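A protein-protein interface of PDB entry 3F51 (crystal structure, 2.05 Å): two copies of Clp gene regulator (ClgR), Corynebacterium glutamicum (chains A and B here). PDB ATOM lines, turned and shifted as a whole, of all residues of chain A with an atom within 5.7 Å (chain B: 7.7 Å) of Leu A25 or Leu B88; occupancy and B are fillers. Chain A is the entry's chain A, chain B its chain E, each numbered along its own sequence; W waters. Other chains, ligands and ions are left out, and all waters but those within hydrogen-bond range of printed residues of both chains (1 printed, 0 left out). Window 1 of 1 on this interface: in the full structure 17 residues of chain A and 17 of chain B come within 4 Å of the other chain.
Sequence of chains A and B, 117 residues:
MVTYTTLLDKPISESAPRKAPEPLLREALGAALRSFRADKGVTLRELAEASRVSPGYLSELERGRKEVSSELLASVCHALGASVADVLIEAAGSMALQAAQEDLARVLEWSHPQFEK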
ATOM      1  N   PRO A  23     -16.232  -3.583 -27.040  1.00  0.00           N
ATOM      2  CA  PRO A  23     -15.316  -2.479 -26.684  1.00  0.00           C
ATOM      3  C   PRO A  23     -15.975  -1.514 -25.725  1.00  0.00           C
ATOM      4  O   PRO A  23     -17.188  -1.323 -25.778  1.00  0.00           O
ATOM      5  CB  PRO A  23     -15.060  -1.777 -28.009  1.00  0.00           C
ATOM      6  CG  PRO A  23     -15.362  -2.830 -29.043  1.00  0.00           C
ATOM      7  CD  PRO A  23     -16.466  -3.655 -28.491  1.00  0.00           C
ATOM      8  N   LEU A  24     -15.183  -0.946 -24.833  1.00  0.00           N
ATOM      9  CA  LEU A  24     -15.700   0.003 -23.889  1.00  0.00           C
ATOM     10  C   LEU A  24     -16.123   1.271 -24.624  1.00  0.00           C
ATOM     11  O   LEU A  24     -15.587   1.605 -25.688  1.00  0.00           O
ATOM     12  CB  LEU A  24     -14.652   0.346 -22.826  1.00  0.00           C
ATOM     13  CG  LEU A  24     -14.205  -0.839 -21.963  1.00  0.00           C
ATOM     14  CD1 LEU A  24     -13.089  -0.375 -21.009  1.00  0.00           C
ATOM     15  CD2 LEU A  24     -15.318  -1.528 -21.196  1.00  0.00           C
ATOM     16  N   LEU A  25     -17.095   1.951 -24.054  1.00  0.00           N
ATOM     17  CA  LEU A  25     -17.559   3.230 -24.586  1.00  0.00           C
ATOM     18  C   LEU A  25     -16.385   4.220 -24.797  1.00  0.00           C
ATOM     19  O   LEU A  25     -16.232   4.762 -25.883  1.00  0.00           O
ATOM     20  CB  LEU A  25     -18.600   3.837 -23.643  1.00  0.00           C
ATOM     21  CG  LEU A  25     -19.169   5.216 -24.087  1.00  0.00           C
ATOM     22  CD1 LEU A  25     -19.725   5.138 -25.513  1.00  0.00           C
ATOM     23  CD2 LEU A  25     -20.229   5.675 -23.140  1.00  0.00           C
ATOM     24  N   ARG A  26     -15.513   4.393 -23.800  1.00  0.00           N
ATOM     25  CA  ARG A  26     -14.466   5.449 -23.942  1.00  0.00           C
ATOM     26  C   ARG A  26     -13.549   5.100 -25.085  1.00  0.00           C
ATOM     27  O   ARG A  26     -12.991   5.995 -25.711  1.00  0.00           O
ATOM     28  CB  ARG A  26     -13.691   5.691 -22.641  1.00  0.00           C
ATOM     29  CG  ARG A  26     -12.997   4.475 -22.060  1.00  0.00           C
ATOM     30  CD  ARG A  26     -12.121   4.806 -20.832  1.00  0.00           C
ATOM     31  NE  ARG A  26     -11.398   3.589 -20.430  1.00  0.00           N
ATOM     32  CZ  ARG A  26     -11.799   2.784 -19.455  1.00  0.00           C
ATOM     33  NH1 ARG A  26     -11.103   1.689 -19.144  1.00  0.00           N
ATOM     34  NH2 ARG A  26     -12.890   3.100 -18.758  1.00  0.00           N
ATOM     35  N   GLU A  27     -13.384   3.800 -25.376  1.00  0.00           N
ATOM     36  CA  GLU A  27     -12.515   3.368 -26.509  1.00  0.00           C
ATOM     37  C   GLU A  27     -13.154   3.702 -27.857  1.00  0.00           C
ATOM     38  O   GLU A  27     -12.531   4.271 -28.777  1.00  0.00           O
ATOM     39  CB  GLU A  27     -12.151   1.870 -26.402  1.00  0.00           C
ATOM     40  N   ALA A  28     -14.417   3.371 -27.964  1.00  0.00           N
ATOM     41  CA  ALA A  28     -15.210   3.702 -29.134  1.00  0.00           C
ATOM     42  C   ALA A  28     -15.325   5.222 -29.375  1.00  0.00           C
ATOM     43  O   ALA A  28     -15.148   5.684 -30.498  1.00  0.00           O
ATOM     44  CB  ALA A  28     -16.650   3.090 -28.932  1.00  0.00           C
ATOM     45  N   LEU A  29     -15.652   5.997 -28.342  1.00  0.00           N
ATOM     46  CA  LEU A  29     -15.766   7.451 -28.517  1.00  0.00           C
ATOM     47  C   LEU A  29     -14.409   8.058 -28.839  1.00  0.00           C
ATOM     48  O   LEU A  29     -14.310   8.966 -29.666  1.00  0.00           O
ATOM     49  CB  LEU A  29     -16.308   8.136 -27.258  1.00  0.00           C
ATOM     50  CG  LEU A  29     -17.745   7.940 -26.868  1.00  0.00           C
ATOM     51  CD1 LEU A  29     -17.847   8.467 -25.424  1.00  0.00           C
ATOM     52  CD2 LEU A  29     -18.614   8.731 -27.837  1.00  0.00           C
ATOM     53  N   GLY A  30     -13.348   7.534 -28.219  1.00  0.00           N
ATOM     54  CA  GLY A  30     -12.020   8.066 -28.499  1.00  0.00           C
ATOM     55  C   GLY A  30     -11.632   7.872 -29.954  1.00  0.00           C
ATOM     56  O   GLY A  30     -11.137   8.816 -30.603  1.00  0.00           O
ATOM     57  N   LEU A  88     -21.630   9.743 -31.425  1.00  0.00           N
ATOM     58  CA  LEU A  88     -22.194   8.513 -30.848  1.00  0.00           C
ATOM     59  C   LEU A  88     -22.508   7.440 -31.861  1.00  0.00           C
ATOM     60  O   LEU A  88     -22.284   6.265 -31.598  1.00  0.00           O
ATOM     61  CB  LEU A  88     -23.458   8.759 -30.049  1.00  0.00           C
ATOM     62  CG  LEU A  88     -23.303   9.811 -28.941  1.00  0.00           C
ATOM     63  CD1 LEU A  88     -24.640   9.882 -28.133  1.00  0.00           C
ATOM     64  CD2 LEU A  88     -22.150   9.382 -28.052  1.00  0.00           C
ATOM     65  N   ILE A  89     -23.084   7.836 -32.991  1.00  0.00           N
ATOM     66  CA  ILE A  89     -23.440   6.869 -34.022  1.00  0.00           C
ATOM     67  C   ILE A  89     -22.170   6.264 -34.587  1.00  0.00           C
ATOM     68  O   ILE A  89     -22.074   5.044 -34.780  1.00  0.00           O
ATOM     69  CB  ILE A  89     -24.312   7.514 -35.129  1.00  0.00           C
ATOM     70  CG1 ILE A  89     -25.705   7.878 -34.568  1.00  0.00           C
ATOM     71  CG2 ILE A  89     -24.440   6.570 -36.312  1.00  0.00           C
ATOM     72  CD1 ILE A  89     -26.618   6.656 -34.103  1.00  0.00           C
ATOM     73  N   ALA A  91     -19.306   5.920 -32.961  1.00  0.00           N
ATOM     74  CA  ALA A  91     -18.827   5.056 -31.927  1.00  0.00           C
ATOM     75  C   ALA A  91     -19.631   3.749 -31.874  1.00  0.00           C
ATOM     76  O   ALA A  91     -19.067   2.675 -31.665  1.00  0.00           O
ATOM     77  CB  ALA A  91     -18.903   5.790 -30.540  1.00  0.00           C
ATOM     78  N   ALA A  92     -20.936   3.807 -32.075  1.00  0.00           N
ATOM     79  CA  ALA A  92     -21.750   2.605 -31.916  1.00  0.00           C
ATOM     80  C   ALA A  92     -21.505   1.684 -33.114  1.00  0.00           C
ATOM     81  O   ALA A  92     -21.406   0.465 -32.971  1.00  0.00           O
ATOM     82  CB  ALA A  92     -23.177   2.972 -31.823  1.00  0.00           C
ATOM     83  N   MET A  95     -18.056   0.090 -32.563  1.00  0.00           N
ATOM     84  CA  MET A  95     -18.172  -0.924 -31.536  1.00  0.00           C
ATOM     85  C   MET A  95     -18.719  -2.208 -32.093  1.00  0.00           C
ATOM     86  O   MET A  95     -18.168  -3.265 -31.818  1.00  0.00           O
ATOM     87  CB  MET A  95     -19.090  -0.494 -30.393  1.00  0.00           C
ATOM     88  CG  MET A  95     -18.435   0.582 -29.564  1.00  0.00           C
ATOM     89  SD  MET A  95     -19.591   1.226 -28.322  1.00  0.00           S
ATOM     90  CE  MET A  95     -20.130  -0.314 -27.575  1.00  0.00           C
ATOM     91  N   LEU B  25     -24.512  14.095 -22.999  1.00  0.00           N
ATOM     92  CA  LEU B  25     -24.444  12.641 -23.149  1.00  0.00           C
ATOM     93  C   LEU B  25     -25.011  11.903 -21.920  1.00  0.00           C
ATOM     94  O   LEU B  25     -25.808  11.003 -22.079  1.00  0.00           O
ATOM     95  CB  LEU B  25     -23.035  12.158 -23.483  1.00  0.00           C
ATOM     96  CG  LEU B  25     -22.808  10.619 -23.537  1.00  0.00           C
ATOM     97  CD1 LEU B  25     -23.677  10.010 -24.602  1.00  0.00           C
ATOM     98  CD2 LEU B  25     -21.339  10.299 -23.780  1.00  0.00           C
ATOM     99  N   ALA B  28     -28.877  12.032 -22.162  1.00  0.00           N
ATOM    100  CA  ALA B  28     -29.404  11.144 -23.203  1.00  0.00           C
ATOM    101  C   ALA B  28     -29.140   9.664 -22.863  1.00  0.00           C
ATOM    102  O   ALA B  28     -30.015   8.817 -23.086  1.00  0.00           O
ATOM    103  CB  ALA B  28     -28.759  11.486 -24.558  1.00  0.00           C
ATOM    104  N   LEU B  29     -27.953   9.339 -22.347  1.00  0.00           N
ATOM    105  CA  LEU B  29     -27.675   7.936 -21.957  1.00  0.00           C
ATOM    106  C   LEU B  29     -28.585   7.458 -20.843  1.00  0.00           C
ATOM    107  O   LEU B  29     -29.057   6.338 -20.887  1.00  0.00           O
ATOM    108  CB  LEU B  29     -26.244   7.744 -21.482  1.00  0.00           C
ATOM    109  CG  LEU B  29     -25.270   7.291 -22.557  1.00  0.00           C
ATOM    110  CD1 LEU B  29     -23.877   7.333 -21.964  1.00  0.00           C
ATOM    111  CD2 LEU B  29     -25.673   5.876 -23.013  1.00  0.00           C
ATOM    112  N   ALA B  32     -31.999   6.839 -22.258  1.00  0.00           N
ATOM    113  CA  ALA B  32     -31.979   5.559 -22.983  1.00  0.00           C
ATOM    114  C   ALA B  32     -31.976   4.347 -22.020  1.00  0.00           C
ATOM    115  O   ALA B  32     -32.711   3.391 -22.205  1.00  0.00           O
ATOM    116  CB  ALA B  32     -30.800   5.477 -23.889  1.00  0.00           C
ATOM    117  N   PHE B  36     -34.766   1.285 -21.869  1.00  0.00           N
ATOM    118  CA  PHE B  36     -34.486  -0.151 -21.903  1.00  0.00           C
ATOM    119  C   PHE B  36     -35.010  -0.857 -20.661  1.00  0.00           C
ATOM    120  O   PHE B  36     -35.605  -1.946 -20.703  1.00  0.00           O
ATOM    121  CB  PHE B  36     -33.000  -0.368 -22.086  1.00  0.00           C
ATOM    122  CG  PHE B  36     -32.575  -0.312 -23.522  1.00  0.00           C
ATOM    123  CD1 PHE B  36     -32.416   0.919 -24.169  1.00  0.00           C
ATOM    124  CD2 PHE B  36     -32.315  -1.477 -24.231  1.00  0.00           C
ATOM    125  CE1 PHE B  36     -32.034   1.004 -25.534  1.00  0.00           C
ATOM    126  CE2 PHE B  36     -31.908  -1.389 -25.621  1.00  0.00           C
ATOM    127  CZ  PHE B  36     -31.793  -0.148 -26.239  1.00  0.00           C
ATOM    128  N   VAL B  68     -21.050   8.093 -15.756  1.00  0.00           N
ATOM    129  CA  VAL B  68     -20.835   6.652 -15.490  1.00  0.00           C
ATOM    130  C   VAL B  68     -19.525   6.165 -16.168  1.00  0.00           C
ATOM    131  O   VAL B  68     -19.214   6.593 -17.273  1.00  0.00           O
ATOM    132  CB  VAL B  68     -22.083   5.855 -15.934  1.00  0.00           C
ATOM    133  CG1 VAL B  68     -22.401   6.036 -17.445  1.00  0.00           C
ATOM    134  CG2 VAL B  68     -22.015   4.381 -15.557  1.00  0.00           C
ATOM    135  N   SER B  69     -18.743   5.302 -15.518  1.00  0.00           N
ATOM    136  CA  SER B  69     -17.576   4.734 -16.209  1.00  0.00           C
ATOM    137  C   SER B  69     -18.074   3.789 -17.318  1.00  0.00           C
ATOM    138  O   SER B  69     -19.171   3.239 -17.216  1.00  0.00           O
ATOM    139  CB  SER B  69     -16.698   3.969 -15.234  1.00  0.00           C
ATOM    140  OG  SER B  69     -17.362   2.784 -14.798  1.00  0.00           O
ATOM    141  N   SER B  70     -17.275   3.604 -18.365  1.00  0.00           N
ATOM    142  CA  SER B  70     -17.566   2.606 -19.420  1.00  0.00           C
ATOM    143  C   SER B  70     -17.830   1.151 -18.907  1.00  0.00           C
ATOM    144  O   SER B  70     -18.688   0.439 -19.449  1.00  0.00           O
ATOM    145  CB  SER B  70     -16.441   2.596 -20.457  1.00  0.00           C
ATOM    146  OG  SER B  70     -16.278   3.890 -21.079  1.00  0.00           O
ATOM    147  N   GLU B  71     -17.108   0.740 -17.860  1.00  0.00           N
ATOM    148  CA  GLU B  71     -17.234  -0.606 -17.279  1.00  0.00           C
ATOM    149  C   GLU B  71     -18.588  -0.806 -16.625  1.00  0.00           C
ATOM    150  O   GLU B  71     -19.239  -1.842 -16.798  1.00  0.00           O
ATOM    151  CB  GLU B  71     -16.116  -0.823 -16.253  1.00  0.00           C
ATOM    152  CG  GLU B  71     -14.755  -1.057 -16.898  1.00  0.00           C
ATOM    153  CD  GLU B  71     -13.934   0.202 -17.112  1.00  0.00           C
ATOM    154  OE1 GLU B  71     -14.432   1.344 -16.917  1.00  0.00           O
ATOM    155  OE2 GLU B  71     -12.748   0.041 -17.493  1.00  0.00           O
ATOM    156  N   LEU B  73     -21.291   1.130 -17.262  1.00  0.00           N
ATOM    157  CA  LEU B  73     -22.253   1.190 -18.384  1.00  0.00           C
ATOM    158  C   LEU B  73     -22.447  -0.174 -19.041  1.00  0.00           C
ATOM    159  O   LEU B  73     -23.566  -0.583 -19.318  1.00  0.00           O
ATOM    160  CB  LEU B  73     -21.785   2.199 -19.444  1.00  0.00           C
ATOM    161  CG  LEU B  73     -22.760   2.373 -20.614  1.00  0.00           C
ATOM    162  CD1 LEU B  73     -24.222   2.593 -20.142  1.00  0.00           C
ATOM    163  CD2 LEU B  73     -22.261   3.513 -21.509  1.00  0.00           C
ATOM    164  N   ALA B  74     -21.349  -0.879 -19.263  1.00  0.00           N
ATOM    165  CA  ALA B  74     -21.380  -2.195 -19.879  1.00  0.00           C
ATOM    166  C   ALA B  74     -22.160  -3.184 -19.014  1.00  0.00           C
ATOM    167  O   ALA B  74     -22.993  -3.898 -19.515  1.00  0.00           O
ATOM    168  CB  ALA B  74     -19.939  -2.700 -20.145  1.00  0.00           C
ATOM    169  N   CYS B  77     -25.941  -2.346 -19.115  1.00  0.00           N
ATOM    170  CA  CYS B  77     -26.569  -2.683 -20.393  1.00  0.00           C
ATOM    171  C   CYS B  77     -26.710  -4.195 -20.494  1.00  0.00           C
ATOM    172  O   CYS B  77     -27.774  -4.717 -20.838  1.00  0.00           O
ATOM    173  CB  CYS B  77     -25.724  -2.143 -21.549  1.00  0.00           C
ATOM    174  SG  CYS B  77     -25.791  -0.355 -21.619  1.00  0.00           S
ATOM    175  N   SER B  83     -26.785  -4.646 -25.906  1.00  0.00           N
ATOM    176  CA  SER B  83     -25.422  -4.205 -26.164  1.00  0.00           C
ATOM    177  C   SER B  83     -25.311  -2.751 -25.815  1.00  0.00           C
ATOM    178  O   SER B  83     -26.284  -1.999 -25.932  1.00  0.00           O
ATOM    179  CB  SER B  83     -25.071  -4.353 -27.642  1.00  0.00           C
ATOM    180  OG  SER B  83     -25.906  -3.499 -28.387  1.00  0.00           O
ATOM    181  N   VAL B  84     -24.109  -2.330 -25.420  1.00  0.00           N
ATOM    182  CA  VAL B  84     -23.863  -0.896 -25.196  1.00  0.00           C
ATOM    183  C   VAL B  84     -24.134  -0.113 -26.469  1.00  0.00           C
ATOM    184  O   VAL B  84     -24.696   0.977 -26.431  1.00  0.00           O
ATOM    185  CB  VAL B  84     -22.473  -0.645 -24.610  1.00  0.00           C
ATOM    186  CG1 VAL B  84     -22.215   0.867 -24.455  1.00  0.00           C
ATOM    187  CG2 VAL B  84     -22.494  -1.339 -23.239  1.00  0.00           C
ATOM    188  N   ALA B  85     -23.798  -0.727 -27.585  1.00  0.00           N
ATOM    189  CA  ALA B  85     -23.956  -0.072 -28.869  1.00  0.00           C
ATOM    190  C   ALA B  85     -25.434   0.230 -29.177  1.00  0.00           C
ATOM    191  O   ALA B  85     -25.745   1.340 -29.624  1.00  0.00           O
ATOM    192  CB  ALA B  85     -23.270  -0.899 -29.987  1.00  0.00           C
ATOM    193  N   ASP B  86     -26.352  -0.697 -28.883  1.00  0.00           N
ATOM    194  CA  ASP B  86     -27.795  -0.397 -28.991  1.00  0.00           C
ATOM    195  C   ASP B  86     -28.285   0.718 -28.066  1.00  0.00           C
ATOM    196  O   ASP B  86     -29.106   1.523 -28.475  1.00  0.00           O
ATOM    197  CB  ASP B  86     -28.662  -1.642 -28.802  1.00  0.00           C
ATOM    198  CG  ASP B  86     -28.480  -2.612 -29.954  1.00  0.00           C
ATOM    199  OD1 ASP B  86     -28.185  -2.154 -31.115  1.00  0.00           O
ATOM    200  OD2 ASP B  86     -28.554  -3.810 -29.686  1.00  0.00           O
ATOM    201  N   VAL B  87     -27.820   0.740 -26.820  1.00  0.00           N
ATOM    202  CA  VAL B  87     -28.218   1.821 -25.916  1.00  0.00           C
ATOM    203  C   VAL B  87     -27.670   3.187 -26.440  1.00  0.00           C
ATOM    204  O   VAL B  87     -28.309   4.236 -26.319  1.00  0.00           O
ATOM    205  CB  VAL B  87     -27.742   1.522 -24.477  1.00  0.00           C
ATOM    206  CG1 VAL B  87     -28.060   2.727 -23.564  1.00  0.00           C
ATOM    207  CG2 VAL B  87     -28.504   0.261 -23.952  1.00  0.00           C
ATOM    208  N   LEU B  88     -26.505   3.161 -27.067  1.00  0.00           N
ATOM    209  CA  LEU B  88     -25.931   4.371 -27.584  1.00  0.00           C
ATOM    210  C   LEU B  88     -26.669   4.872 -28.828  1.00  0.00           C
ATOM    211  O   LEU B  88     -26.791   6.073 -29.064  1.00  0.00           O
ATOM    212  CB  LEU B  88     -24.482   4.122 -27.963  1.00  0.00           C
ATOM    213  CG  LEU B  88     -23.359   4.460 -26.984  1.00  0.00           C
ATOM    214  CD1 LEU B  88     -21.998   4.455 -27.728  1.00  0.00           C
ATOM    215  CD2 LEU B  88     -23.539   5.856 -26.354  1.00  0.00           C
ATOM    216  N   ILE B  89     -27.118   3.953 -29.658  1.00  0.00           N
ATOM    217  CA  ILE B  89     -27.923   4.346 -30.811  1.00  0.00           C
ATOM    218  C   ILE B  89     -29.219   5.024 -30.314  1.00  0.00           C
ATOM    219  O   ILE B  89     -29.630   6.068 -30.802  1.00  0.00           O
ATOM    220  CB  ILE B  89     -28.151   3.169 -31.733  1.00  0.00           C
ATOM    221  CG1 ILE B  89     -26.839   2.788 -32.467  1.00  0.00           C
ATOM    222  CG2 ILE B  89     -29.309   3.444 -32.727  1.00  0.00           C
ATOM    223  CD1 ILE B  89     -26.913   1.342 -33.078  1.00  0.00           C
ATOM    224  N   GLU B  90     -29.855   4.444 -29.320  1.00  0.00           N
ATOM    225  CA  GLU B  90     -31.065   5.033 -28.759  1.00  0.00           C
ATOM    226  C   GLU B  90     -30.780   6.422 -28.138  1.00  0.00           C
ATOM    227  O   GLU B  90     -31.595   7.347 -28.250  1.00  0.00           O
ATOM    228  CB  GLU B  90     -31.575   4.126 -27.661  1.00  0.00           C
ATOM    229  CG  GLU B  90     -32.639   4.745 -26.821  1.00  0.00           C
ATOM    230  CD  GLU B  90     -33.977   4.865 -27.524  1.00  0.00           C
ATOM    231  OE1 GLU B  90     -34.879   5.577 -26.979  1.00  0.00           O
ATOM    232  OE2 GLU B  90     -34.129   4.255 -28.600  1.00  0.00           O
ATOM    233  N   ALA B  91     -29.651   6.529 -27.427  1.00  0.00           N
ATOM    234  CA  ALA B  91     -29.207   7.786 -26.837  1.00  0.00           C
ATOM    235  C   ALA B  91     -28.970   8.854 -27.892  1.00  0.00           C
ATOM    236  O   ALA B  91     -29.343  10.006 -27.680  1.00  0.00           O
ATOM    237  CB  ALA B  91     -27.908   7.571 -25.971  1.00  0.00           C
ATOM    238  N   ALA B  92     -28.352   8.484 -29.017  1.00  0.00           N
ATOM    239  CA  ALA B  92     -28.083   9.399 -30.106  1.00  0.00           C
ATOM    240  C   ALA B  92     -29.385   9.896 -30.766  1.00  0.00           C
ATOM    241  O   ALA B  92     -29.521  11.090 -31.082  1.00  0.00           O
ATOM    242  CB  ALA B  92     -27.153   8.735 -31.160  1.00  0.00           C
ATOM    243  N   GLY B  93     -30.320   8.983 -31.018  1.00  0.00           N
ATOM    244  CA  GLY B  93     -31.610   9.345 -31.600  1.00  0.00           C
ATOM    245  C   GLY B  93     -32.356  10.286 -30.658  1.00  0.00           C
ATOM    246  O   GLY B  93     -32.830  11.356 -31.060  1.00  0.00           O
ATOM    247  N   SER B  94     -32.376   9.952 -29.386  1.00  0.00           N
ATOM    248  CA  SER B  94     -32.956  10.854 -28.413  1.00  0.00           C
ATOM    249  C   SER B  94     -32.315  12.299 -28.308  1.00  0.00           C
ATOM    250  O   SER B  94     -33.054  13.312 -28.244  1.00  0.00           O
ATOM    251  CB  SER B  94     -32.938  10.133 -27.083  1.00  0.00           C
ATOM    252  OG  SER B  94     -33.383  10.972 -26.045  1.00  0.00           O
ATOM    253  N   MET B  95     -30.981  12.391 -28.304  1.00  0.00           N
ATOM    254  CA  MET B  95     -30.292  13.668 -28.320  1.00  0.00           C
ATOM    255  C   MET B  95     -30.644  14.464 -29.561  1.00  0.00           C
ATOM    256  O   MET B  95     -30.877  15.664 -29.489  1.00  0.00           O
ATOM    257  CB  MET B  95     -28.739  13.540 -28.325  1.00  0.00           C
ATOM    258  CG  MET B  95     -28.061  12.735 -27.183  1.00  0.00           C
ATOM    259  SD  MET B  95     -26.336  13.351 -26.879  1.00  0.00           S
ATOM    260  CE  MET B  95     -26.105  14.112 -28.410  1.00  0.00           C
HETATM  261  O   HOH W   1     -18.821   0.646 -22.226  1.00  0.00           O
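Among the printed residues, pairs that only touch across the chains: Leu A24 with Ser B70 (3.7 Å), Leu A24 with Glu B71 (3.6 Å), Leu A25 with Ser B70 (3.5 Å), Leu A25 with Leu B73 (3.4 Å), Leu A25 with Leu B88 (3.2 Å), Leu A88 with Leu B25 (3.7 Å), Leu A88 with Ala B92 (3.9 Å), Ile A89 with Ala B92 (3.6 Å), Ala A92 with Ala B85 (3.8 Å), Ala A92 with Ile B89 (3.7 Å), Met A95 with Val B84 (3.8 Å) and Met A95 with Ala B85 (3.7 Å).
Leu A25 touches Leu B88, and with the chains exchanged Leu A88 touches Leu B25.
Leu A88 touches Ala B92, but with the chains exchanged Ala A92 does not touch Leu B88 (4.2 Å).
Ile A89 touches Ala B92, and with the chains exchanged Ala A92 touches Ile B89.
8 positions are printed for both chains.
Water W1 bridges the backbone carbonyl oxygen (O) of Ser B70 and the backbone NH (N) of Leu A25.
The side-chain hydroxyl (OG) of Ser B70 lies within hydrogen-bond range of the backbone NH (N) of Arg A26, 2.9 Å away.
NH1 of Arg A26 is in salt-bridge range of OE2 of Glu B71 (2.9 Å).
Printed residues of chain B within 4 Å of Leu A25: Ser B70 (3.5 Å), Leu B73 (3.4 Å) and Leu B88 (3.2 Å).
Of the printed residues of chain A, Ala B85 touches Ala A92 and Met A95.
Printed residues of chain A within 4 Å of Leu B73: Leu A25 (3.4 Å).
The nearest residue of chain B that does not touch Leu A25 is Leu B29 (4.2 Å).
The nearest residue of chain A that does not touch Leu B88 is Met A95 (4.1 Å).
The nearest printed residue of chain B that does not touch Arg A26 is Ser B69 (5.3 Å).
The backbone carbonyl oxygen of Leu B73 lies within hydrogen-bond range of the side-chain sulfur of Cys B77 (3.2 Å).
Of the 13 printed residues of chain A, 7 touch a printed residue of chain B.
Hydrophobic or aromatic side chains of chain A within 4 Å of the printed part of chain B: Leu A24, Leu A25, Leu A88, Ile A89, Ala A92 and Met A95.
Of the 25 printed residues of chain B, 9 touch a printed residue of chain A.
Hydrophobic or aromatic side chains of chain B that line the printed part of chain A: Leu B25, Leu B73, Val B84, Ala B85, Leu B88, Ile B89 and Ala B92.
Along chain B the printed residues that touch a printed residue of chain A span positions 25 to 92.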
